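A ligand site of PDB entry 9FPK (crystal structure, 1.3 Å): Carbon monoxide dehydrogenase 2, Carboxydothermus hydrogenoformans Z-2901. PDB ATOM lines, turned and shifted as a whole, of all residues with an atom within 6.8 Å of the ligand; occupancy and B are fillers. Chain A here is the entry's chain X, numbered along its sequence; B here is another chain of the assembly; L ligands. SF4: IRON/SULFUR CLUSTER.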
ATOM      1  N   CYS A  47      13.210  -8.072  11.918  1.00  0.00           N
ATOM      2  CA  CYS A  47      12.468  -6.831  11.719  1.00  0.00           C
ATOM      3  C   CYS A  47      12.790  -6.345  10.318  1.00  0.00           C
ATOM      4  O   CYS A  47      13.926  -6.467   9.858  1.00  0.00           O
ATOM      5  CB  CYS A  47      12.875  -5.774  12.739  1.00  0.00           C
ATOM      6  SG  CYS A  47      12.035  -4.168  12.421  1.00  0.00           S
ATOM      7  N   CYS A  48      11.765  -5.824   9.633  1.00  0.00           N
ATOM      8  CA  CYS A  48      11.936  -5.281   8.292  1.00  0.00           C
ATOM      9  C   CYS A  48      11.191  -3.968   8.191  1.00  0.00           C
ATOM     10  O   CYS A  48      10.027  -3.891   8.599  1.00  0.00           O
ATOM     11  CB  CYS A  48      11.444  -6.286   7.278  1.00  0.00           C
ATOM     12  SG  CYS A  48      11.574  -5.653   5.557  1.00  0.00           S
ATOM     13  N   ARG A  49      11.857  -2.955   7.634  1.00  0.00           N
ATOM     14  CA  ARG A  49      11.285  -1.636   7.355  1.00  0.00           C
ATOM     15  C   ARG A  49      11.519  -1.268   5.885  1.00  0.00           C
ATOM     16  O   ARG A  49      11.676  -0.092   5.545  1.00  0.00           O
ATOM     17  CB  ARG A  49      11.815  -0.558   8.300  1.00  0.00           C
ATOM     18  CG  ARG A  49      11.511  -0.858   9.739  1.00  0.00           C
ATOM     19  CD  ARG A  49      12.315   0.018  10.696  1.00  0.00           C
ATOM     20  NE  ARG A  49      12.063   1.406  10.418  1.00  0.00           N
ATOM     21  CZ  ARG A  49      12.859   2.429  10.678  1.00  0.00           C
ATOM     22  NH1 ARG A  49      13.992   2.268  11.327  1.00  0.00           N
ATOM     23  NH2 ARG A  49      12.454   3.659  10.318  1.00  0.00           N
ATOM     24  N   HIS A  50      11.564  -2.275   5.018  1.00  0.00           N
ATOM     25  CA  HIS A  50      11.864  -1.992   3.620  1.00  0.00           C
ATOM     26  C   HIS A  50      10.674  -1.486   2.804  1.00  0.00           C
ATOM     27  O   HIS A  50      10.880  -1.165   1.631  1.00  0.00           O
ATOM     28  CB  HIS A  50      12.501  -3.182   2.922  1.00  0.00           C
ATOM     29  CG  HIS A  50      13.847  -3.583   3.451  1.00  0.00           C
ATOM     30  ND1 HIS A  50      14.695  -4.423   2.778  1.00  0.00           N
ATOM     31  CD2 HIS A  50      14.480  -3.248   4.607  1.00  0.00           C
ATOM     32  CE1 HIS A  50      15.804  -4.608   3.503  1.00  0.00           C
ATOM     33  NE2 HIS A  50      15.700  -3.900   4.606  1.00  0.00           N
ATOM     34  N   CYS A  51       9.508  -1.300   3.402  1.00  0.00           N
ATOM     35  CA  CYS A  51       8.434  -0.602   2.711  1.00  0.00           C
ATOM     36  C   CYS A  51       7.501   0.023   3.729  1.00  0.00           C
ATOM     37  O   CYS A  51       7.576  -0.223   4.940  1.00  0.00           O
ATOM     38  CB  CYS A  51       7.663  -1.488   1.725  1.00  0.00           C
ATOM     39  SG  CYS A  51       6.381  -2.544   2.436  1.00  0.00           S
ATOM     40  N   LEU A  52       6.587   0.846   3.226  1.00  0.00           N
ATOM     41  CA  LEU A  52       5.699   1.596   4.106  1.00  0.00           C
ATOM     42  C   LEU A  52       4.494   0.802   4.584  1.00  0.00           C
ATOM     43  O   LEU A  52       3.638   1.356   5.299  1.00  0.00           O
ATOM     44  CB  LEU A  52       5.240   2.885   3.436  1.00  0.00           C
ATOM     45  CG  LEU A  52       6.328   3.839   2.978  1.00  0.00           C
ATOM     46  CD1 LEU A  52       5.733   5.060   2.278  1.00  0.00           C
ATOM     47  CD2 LEU A  52       7.194   4.245   4.140  1.00  0.00           C
ATOM     48  N   GLN A  53       4.426  -0.494   4.294  1.00  0.00           N
ATOM     49  CA  GLN A  53       3.494  -1.353   4.979  1.00  0.00           C
ATOM     50  C   GLN A  53       4.050  -1.770   6.326  1.00  0.00           C
ATOM     51  O   GLN A  53       3.294  -2.204   7.187  1.00  0.00           O
ATOM     52  CB  GLN A  53       3.154  -2.584   4.134  1.00  0.00           C
ATOM     53  CG  GLN A  53       2.340  -2.204   2.928  1.00  0.00           C
ATOM     54  CD  GLN A  53       1.883  -3.355   2.038  1.00  0.00           C
ATOM     55  OE1 GLN A  53       0.905  -3.226   1.313  1.00  0.00           O
ATOM     56  NE2 GLN A  53       2.615  -4.469   2.065  1.00  0.00           N
ATOM     57  N   GLY A  54       5.360  -1.692   6.511  1.00  0.00           N
ATOM     58  CA  GLY A  54       5.948  -1.991   7.782  1.00  0.00           C
ATOM     59  C   GLY A  54       5.742  -0.922   8.812  1.00  0.00           C
ATOM     60  O   GLY A  54       5.031   0.067   8.629  1.00  0.00           O
ATOM     61  N   PRO A  55       6.410  -1.098   9.944  1.00  0.00           N
ATOM     62  CA  PRO A  55       7.417  -2.118  10.249  1.00  0.00           C
ATOM     63  C   PRO A  55       6.808  -3.467  10.459  1.00  0.00           C
ATOM     64  O   PRO A  55       5.720  -3.634  11.033  1.00  0.00           O
ATOM     65  CB  PRO A  55       8.034  -1.582  11.545  1.00  0.00           C
ATOM     66  CG  PRO A  55       6.924  -0.833  12.212  1.00  0.00           C
ATOM     67  CD  PRO A  55       6.190  -0.176  11.079  1.00  0.00           C
ATOM     68  N   CYS A  56       7.517  -4.450   9.922  1.00  0.00           N
ATOM     69  CA  CYS A  56       7.179  -5.843  10.126  1.00  0.00           C
ATOM     70  C   CYS A  56       8.178  -6.485  11.057  1.00  0.00           C
ATOM     71  O   CYS A  56       9.356  -6.126  11.085  1.00  0.00           O
ATOM     72  CB  CYS A  56       7.193  -6.607   8.809  1.00  0.00           C
ATOM     73  SG  CYS A  56       5.833  -6.155   7.718  1.00  0.00           S
ATOM     74  N   ARG A  57       7.720  -7.493  11.783  1.00  0.00           N
ATOM     75  CA  ARG A  57       8.564  -8.254  12.687  1.00  0.00           C
ATOM     76  C   ARG A  57       8.055  -9.673  12.682  1.00  0.00           C
ATOM     77  O   ARG A  57       6.928  -9.957  12.257  1.00  0.00           O
ATOM     78  CB  ARG A  57       8.525  -7.659  14.109  1.00  0.00           C
ATOM     79  CG  ARG A  57       7.212  -7.883  14.806  1.00  0.00           C
ATOM     80  CD  ARG A  57       6.991  -6.984  16.007  1.00  0.00           C
ATOM     81  NE  ARG A  57       5.757  -7.317  16.694  1.00  0.00           N
ATOM     82  CZ  ARG A  57       4.548  -7.087  16.193  1.00  0.00           C
ATOM     83  NH1 ARG A  57       4.372  -6.307  15.138  1.00  0.00           N
ATOM     84  NH2 ARG A  57       3.482  -7.650  16.782  1.00  0.00           N
ATOM     85  N   VAL A  67       5.433 -14.100   9.700  1.00  0.00           N
ATOM     86  CA  VAL A  67       5.810 -13.818   8.327  1.00  0.00           C
ATOM     87  C   VAL A  67       5.541 -12.341   8.104  1.00  0.00           C
ATOM     88  O   VAL A  67       4.619 -11.777   8.696  1.00  0.00           O
ATOM     89  CB  VAL A  67       5.011 -14.730   7.366  1.00  0.00           C
ATOM     90  CG1 VAL A  67       3.505 -14.530   7.548  1.00  0.00           C
ATOM     91  CG2 VAL A  67       5.422 -14.541   5.923  1.00  0.00           C
ATOM     92  N   GLY A  68       6.342 -11.707   7.253  1.00  0.00           N
ATOM     93  CA  GLY A  68       6.117 -10.307   6.947  1.00  0.00           C
ATOM     94  C   GLY A  68       4.825 -10.119   6.168  1.00  0.00           C
ATOM     95  O   GLY A  68       4.271 -11.047   5.586  1.00  0.00           O
ATOM     96  N   ILE A  69       4.365  -8.867   6.101  1.00  0.00           N
ATOM     97  CA  ILE A  69       3.074  -8.572   5.490  1.00  0.00           C
ATOM     98  C   ILE A  69       3.044  -8.979   4.015  1.00  0.00           C
ATOM     99  O   ILE A  69       2.051  -9.525   3.512  1.00  0.00           O
ATOM    100  CB  ILE A  69       2.708  -7.089   5.723  1.00  0.00           C
ATOM    101  CG1 ILE A  69       2.335  -6.863   7.193  1.00  0.00           C
ATOM    102  CG2 ILE A  69       1.595  -6.668   4.794  1.00  0.00           C
ATOM    103  CD1 ILE A  69       2.216  -5.425   7.586  1.00  0.00           C
ATOM    104  N   CYS A  70       4.151  -8.775   3.280  1.00  0.00           N
ATOM    105  CA  CYS A  70       4.218  -9.120   1.869  1.00  0.00           C
ATOM    106  C   CYS A  70       4.446 -10.614   1.641  1.00  0.00           C
ATOM    107  O   CYS A  70       4.494 -11.070   0.494  1.00  0.00           O
ATOM    108  CB  CYS A  70       5.362  -8.370   1.187  1.00  0.00           C
ATOM    109  SG  CYS A  70       6.978  -8.750   1.927  1.00  0.00           S
ATOM    110  N   GLY A  71       4.642 -11.382   2.735  1.00  0.00           N
ATOM    111  CA  GLY A  71       5.014 -12.785   2.654  1.00  0.00           C
ATOM    112  C   GLY A  71       6.477 -13.073   2.895  1.00  0.00           C
ATOM    113  O   GLY A  71       6.879 -14.235   2.835  1.00  0.00           O
ATOM    114  N   ALA A  72       7.292 -12.056   3.179  1.00  0.00           N
ATOM    115  CA  ALA A  72       8.721 -12.279   3.425  1.00  0.00           C
ATOM    116  C   ALA A  72       8.895 -13.156   4.650  1.00  0.00           C
ATOM    117  O   ALA A  72       8.443 -12.829   5.754  1.00  0.00           O
ATOM    118  CB  ALA A  72       9.436 -10.948   3.590  1.00  0.00           C
ATOM    119  N   ILE A  77      13.985 -11.970   5.381  1.00  0.00           N
ATOM    120  CA  ILE A  77      14.180 -10.733   6.123  1.00  0.00           C
ATOM    121  C   ILE A  77      15.591 -10.660   6.695  1.00  0.00           C
ATOM    122  O   ILE A  77      16.273  -9.643   6.559  1.00  0.00           O
ATOM    123  CB  ILE A  77      13.098 -10.600   7.220  1.00  0.00           C
ATOM    124  CG1 ILE A  77      11.754 -10.274   6.581  1.00  0.00           C
ATOM    125  CG2 ILE A  77      13.494  -9.592   8.270  1.00  0.00           C
ATOM    126  CD1 ILE A  77      10.556 -10.306   7.559  1.00  0.00           C
ATOM    127  N   ARG A  80      18.126 -10.183   3.774  1.00  0.00           N
ATOM    128  CA  ARG A  80      18.083  -8.851   3.171  1.00  0.00           C
ATOM    129  C   ARG A  80      18.731  -7.812   4.075  1.00  0.00           C
ATOM    130  O   ARG A  80      19.463  -6.944   3.602  1.00  0.00           O
ATOM    131  CB  ARG A  80      16.646  -8.427   2.842  1.00  0.00           C
ATOM    132  CG  ARG A  80      15.998  -9.293   1.782  1.00  0.00           C
ATOM    133  CD  ARG A  80      14.637  -8.761   1.259  1.00  0.00           C
ATOM    134  NE  ARG A  80      13.683  -8.466   2.327  1.00  0.00           N
ATOM    135  CZ  ARG A  80      12.405  -8.240   2.106  1.00  0.00           C
ATOM    136  NH1 ARG A  80      11.941  -8.258   0.870  1.00  0.00           N
ATOM    137  NH2 ARG A  80      11.580  -8.003   3.123  1.00  0.00           N
ATOM    138  N   THR A 197      17.237  -6.301  -2.494  1.00  0.00           N
ATOM    139  CA  THR A 197      16.712  -6.378  -1.136  1.00  0.00           C
ATOM    140  C   THR A 197      15.506  -5.481  -0.907  1.00  0.00           C
ATOM    141  O   THR A 197      14.911  -5.529   0.173  1.00  0.00           O
ATOM    142  CB  THR A 197      17.766  -6.031  -0.096  1.00  0.00           C
ATOM    143  OG1 THR A 197      18.271  -4.722  -0.368  1.00  0.00           O
ATOM    144  CG2 THR A 197      18.898  -7.070  -0.076  1.00  0.00           C
ATOM    145  N   SER A 198      15.138  -4.674  -1.897  1.00  0.00           N
ATOM    146  CA  SER A 198      13.934  -3.857  -1.792  1.00  0.00           C
ATOM    147  C   SER A 198      12.710  -4.743  -1.923  1.00  0.00           C
ATOM    148  O   SER A 198      12.785  -5.927  -2.279  1.00  0.00           O
ATOM    149  CB  SER A 198      13.962  -2.738  -2.839  1.00  0.00           C
ATOM    150  OG  SER A 198      13.693  -3.175  -4.146  1.00  0.00           O
ATOM    151  N   MET A 199      11.551  -4.167  -1.600  1.00  0.00           N
ATOM    152  CA  MET A 199      10.368  -4.996  -1.476  1.00  0.00           C
ATOM    153  C   MET A 199      10.030  -5.675  -2.794  1.00  0.00           C
ATOM    154  O   MET A 199      10.079  -5.069  -3.886  1.00  0.00           O
ATOM    155  CB  MET A 199       9.196  -4.147  -0.984  1.00  0.00           C
ATOM    156  CG  MET A 199       7.909  -4.932  -0.785  1.00  0.00           C
ATOM    157  SD  MET A 199       6.953  -5.001  -2.354  1.00  0.00           S
ATOM    158  CE  MET A 199       5.800  -6.354  -1.889  1.00  0.00           C
ATOM    159  N   GLY A 200       9.653  -6.958  -2.687  1.00  0.00           N
ATOM    160  CA  GLY A 200       9.134  -7.666  -3.849  1.00  0.00           C
ATOM    161  C   GLY A 200      10.157  -8.042  -4.890  1.00  0.00           C
ATOM    162  O   GLY A 200       9.804  -8.240  -6.057  1.00  0.00           O
ATOM    163  N   MET B  35       0.103  -8.788  12.157  1.00  0.00           N
ATOM    164  CA  MET B  35       1.203  -7.912  12.507  1.00  0.00           C
ATOM    165  C   MET B  35       0.809  -6.827  13.494  1.00  0.00           C
ATOM    166  O   MET B  35       1.681  -6.152  14.055  1.00  0.00           O
ATOM    167  CB  MET B  35       1.761  -7.273  11.228  1.00  0.00           C
ATOM    168  CG  MET B  35       3.167  -6.677  11.389  1.00  0.00           C
ATOM    169  SD  MET B  35       4.389  -7.996  11.791  1.00  0.00           S
ATOM    170  CE  MET B  35       4.553  -8.910  10.346  1.00  0.00           C
ATOM    171  N   GLN B  38       1.626  -2.695  15.163  1.00  0.00           N
ATOM    172  CA  GLN B  38       2.978  -2.583  14.660  1.00  0.00           C
ATOM    173  C   GLN B  38       3.820  -1.690  15.572  1.00  0.00           C
ATOM    174  O   GLN B  38       3.298  -0.907  16.379  1.00  0.00           O
ATOM    175  CB  GLN B  38       2.952  -2.013  13.236  1.00  0.00           C
ATOM    176  CG  GLN B  38       2.342  -2.994  12.260  1.00  0.00           C
ATOM    177  CD  GLN B  38       2.195  -2.446  10.852  1.00  0.00           C
ATOM    178  OE1 GLN B  38       1.236  -1.724  10.575  1.00  0.00           O
ATOM    179  NE2 GLN B  38       3.138  -2.777   9.973  1.00  0.00           N
ATOM    180  N   PRO B 336       6.221 -12.125  -2.117  1.00  0.00           N
ATOM    181  CA  PRO B 336       6.761 -13.486  -2.216  1.00  0.00           C
ATOM    182  C   PRO B 336       5.786 -14.550  -1.769  1.00  0.00           C
ATOM    183  O   PRO B 336       5.996 -15.740  -2.089  1.00  0.00           O
ATOM    184  CB  PRO B 336       8.034 -13.444  -1.365  1.00  0.00           C
ATOM    185  CG  PRO B 336       7.801 -12.289  -0.418  1.00  0.00           C
ATOM    186  CD  PRO B 336       7.065 -11.270  -1.261  1.00  0.00           C
ATOM    187  N   MET B 560       3.724   2.729  -0.971  1.00  0.00           N
ATOM    188  CA  MET B 560       4.273   1.562  -0.278  1.00  0.00           C
ATOM    189  C   MET B 560       5.773   1.413  -0.489  1.00  0.00           C
ATOM    190  O   MET B 560       6.563   1.328   0.451  1.00  0.00           O
ATOM    191  CB  MET B 560       3.534   0.287  -0.747  1.00  0.00           C
ATOM    192  CG  MET B 560       3.983  -1.038  -0.139  1.00  0.00           C
ATOM    193  SD  MET B 560       5.263  -1.877  -1.102  1.00  0.00           S
ATOM    194  CE  MET B 560       4.440  -2.190  -2.674  1.00  0.00           C
HETATM  195 FE1  SF4 L   1       6.922  -5.794   5.706  1.00  0.00          FE
HETATM  196 FE2  SF4 L   1       7.430  -4.221   3.568  1.00  0.00          FE
HETATM  197 FE3  SF4 L   1       9.416  -5.629   4.772  1.00  0.00          FE
HETATM  198 FE4  SF4 L   1       7.563  -6.974   3.330  1.00  0.00          FE
HETATM  199  S1  SF4 L   1       9.099  -5.457   2.564  1.00  0.00           S
HETATM  200  S2  SF4 L   1       8.374  -7.531   5.338  1.00  0.00           S
HETATM  201  S3  SF4 L   1       5.724  -5.698   3.837  1.00  0.00           S
HETATM  202  S4  SF4 L   1       8.205  -3.892   5.642  1.00  0.00           S
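The backbone NH (N) of Cys 51 sits close to a sulfur (S4) of the ligand, 3.7 Å away. An iron atom (FE2) of the ligand is bound by the side-chain sulfur of Cys 51, 2.3 Å away. The side-chain sulfur (SG) of Cys 48 is bound to an iron atom (FE3) of the ligand, at 2.3 Å. An iron atom (FE1) of the ligand is bound by the side-chain sulfur (SG) of Cys 56 (2.3 Å). The backbone NH (N) of Cys 70 lies close to a sulfur (S3) of the ligand, at 3.5 Å. The side-chain sulfur of Cys 70 binds an iron atom (FE4) of the ligand (2.3 Å). The guanidinium group of Arg 80 sits close to a sulfur (S1) of the ligand, 3.6 Å away. S4 of the ligand sits close to N of Gly 54 (3.7 Å). The backbone NH (N) of His 50 lies close to a sulfur (S4) of the ligand (3.8 Å). NE2 of Gln 53 sits close to S3 of the ligand (3.8 Å).
N of Gln 53 sits close to SG of Cys 51 (3.4 Å). The side-chain sulfur (SG) of Cys 51 lies close to the side-chain sulfur (SD) of Met 560 of chain B, at 3.8 Å. The backbone NH (N) of Cys 48 is in hydrogen-bond range of the backbone carbonyl oxygen (O) of Cys 56. The guanidinium group (NH2) of Arg 80 lies close to the side-chain sulfur (SG) of Cys 48 (3.4 Å). O of Cys 56 lies close to SG of Cys 47 (3.6 Å). The backbone NH of Ala 72 lies close to the side-chain sulfur of Cys 70 (3.5 Å). O of Thr 197 sits at hydrogen-bond distance from ND1 of His 50. The side-chain amide nitrogen (NE2) of Gln 38 of chain B lies within hydrogen-bond range of the backbone carbonyl oxygen (O) of Gln 53, at 2.8 Å.
Gly 68 touches the ligand. Ile 69 touches the ligand. Ala 72 touches the ligand (CB to S2, 3.98 Å). CG of Met 199 touches S1 of the ligand, at 3.6 Å. Hydrophobic or aromatic side chains within 4 Å of the ligand: Ile 69, Ala 72 and Met 199. Of the 27 residues printed, 12 come within 4 Å of the ligand. The nearest printed residue that does not touch the ligand is Ile 77 (4.2 Å).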
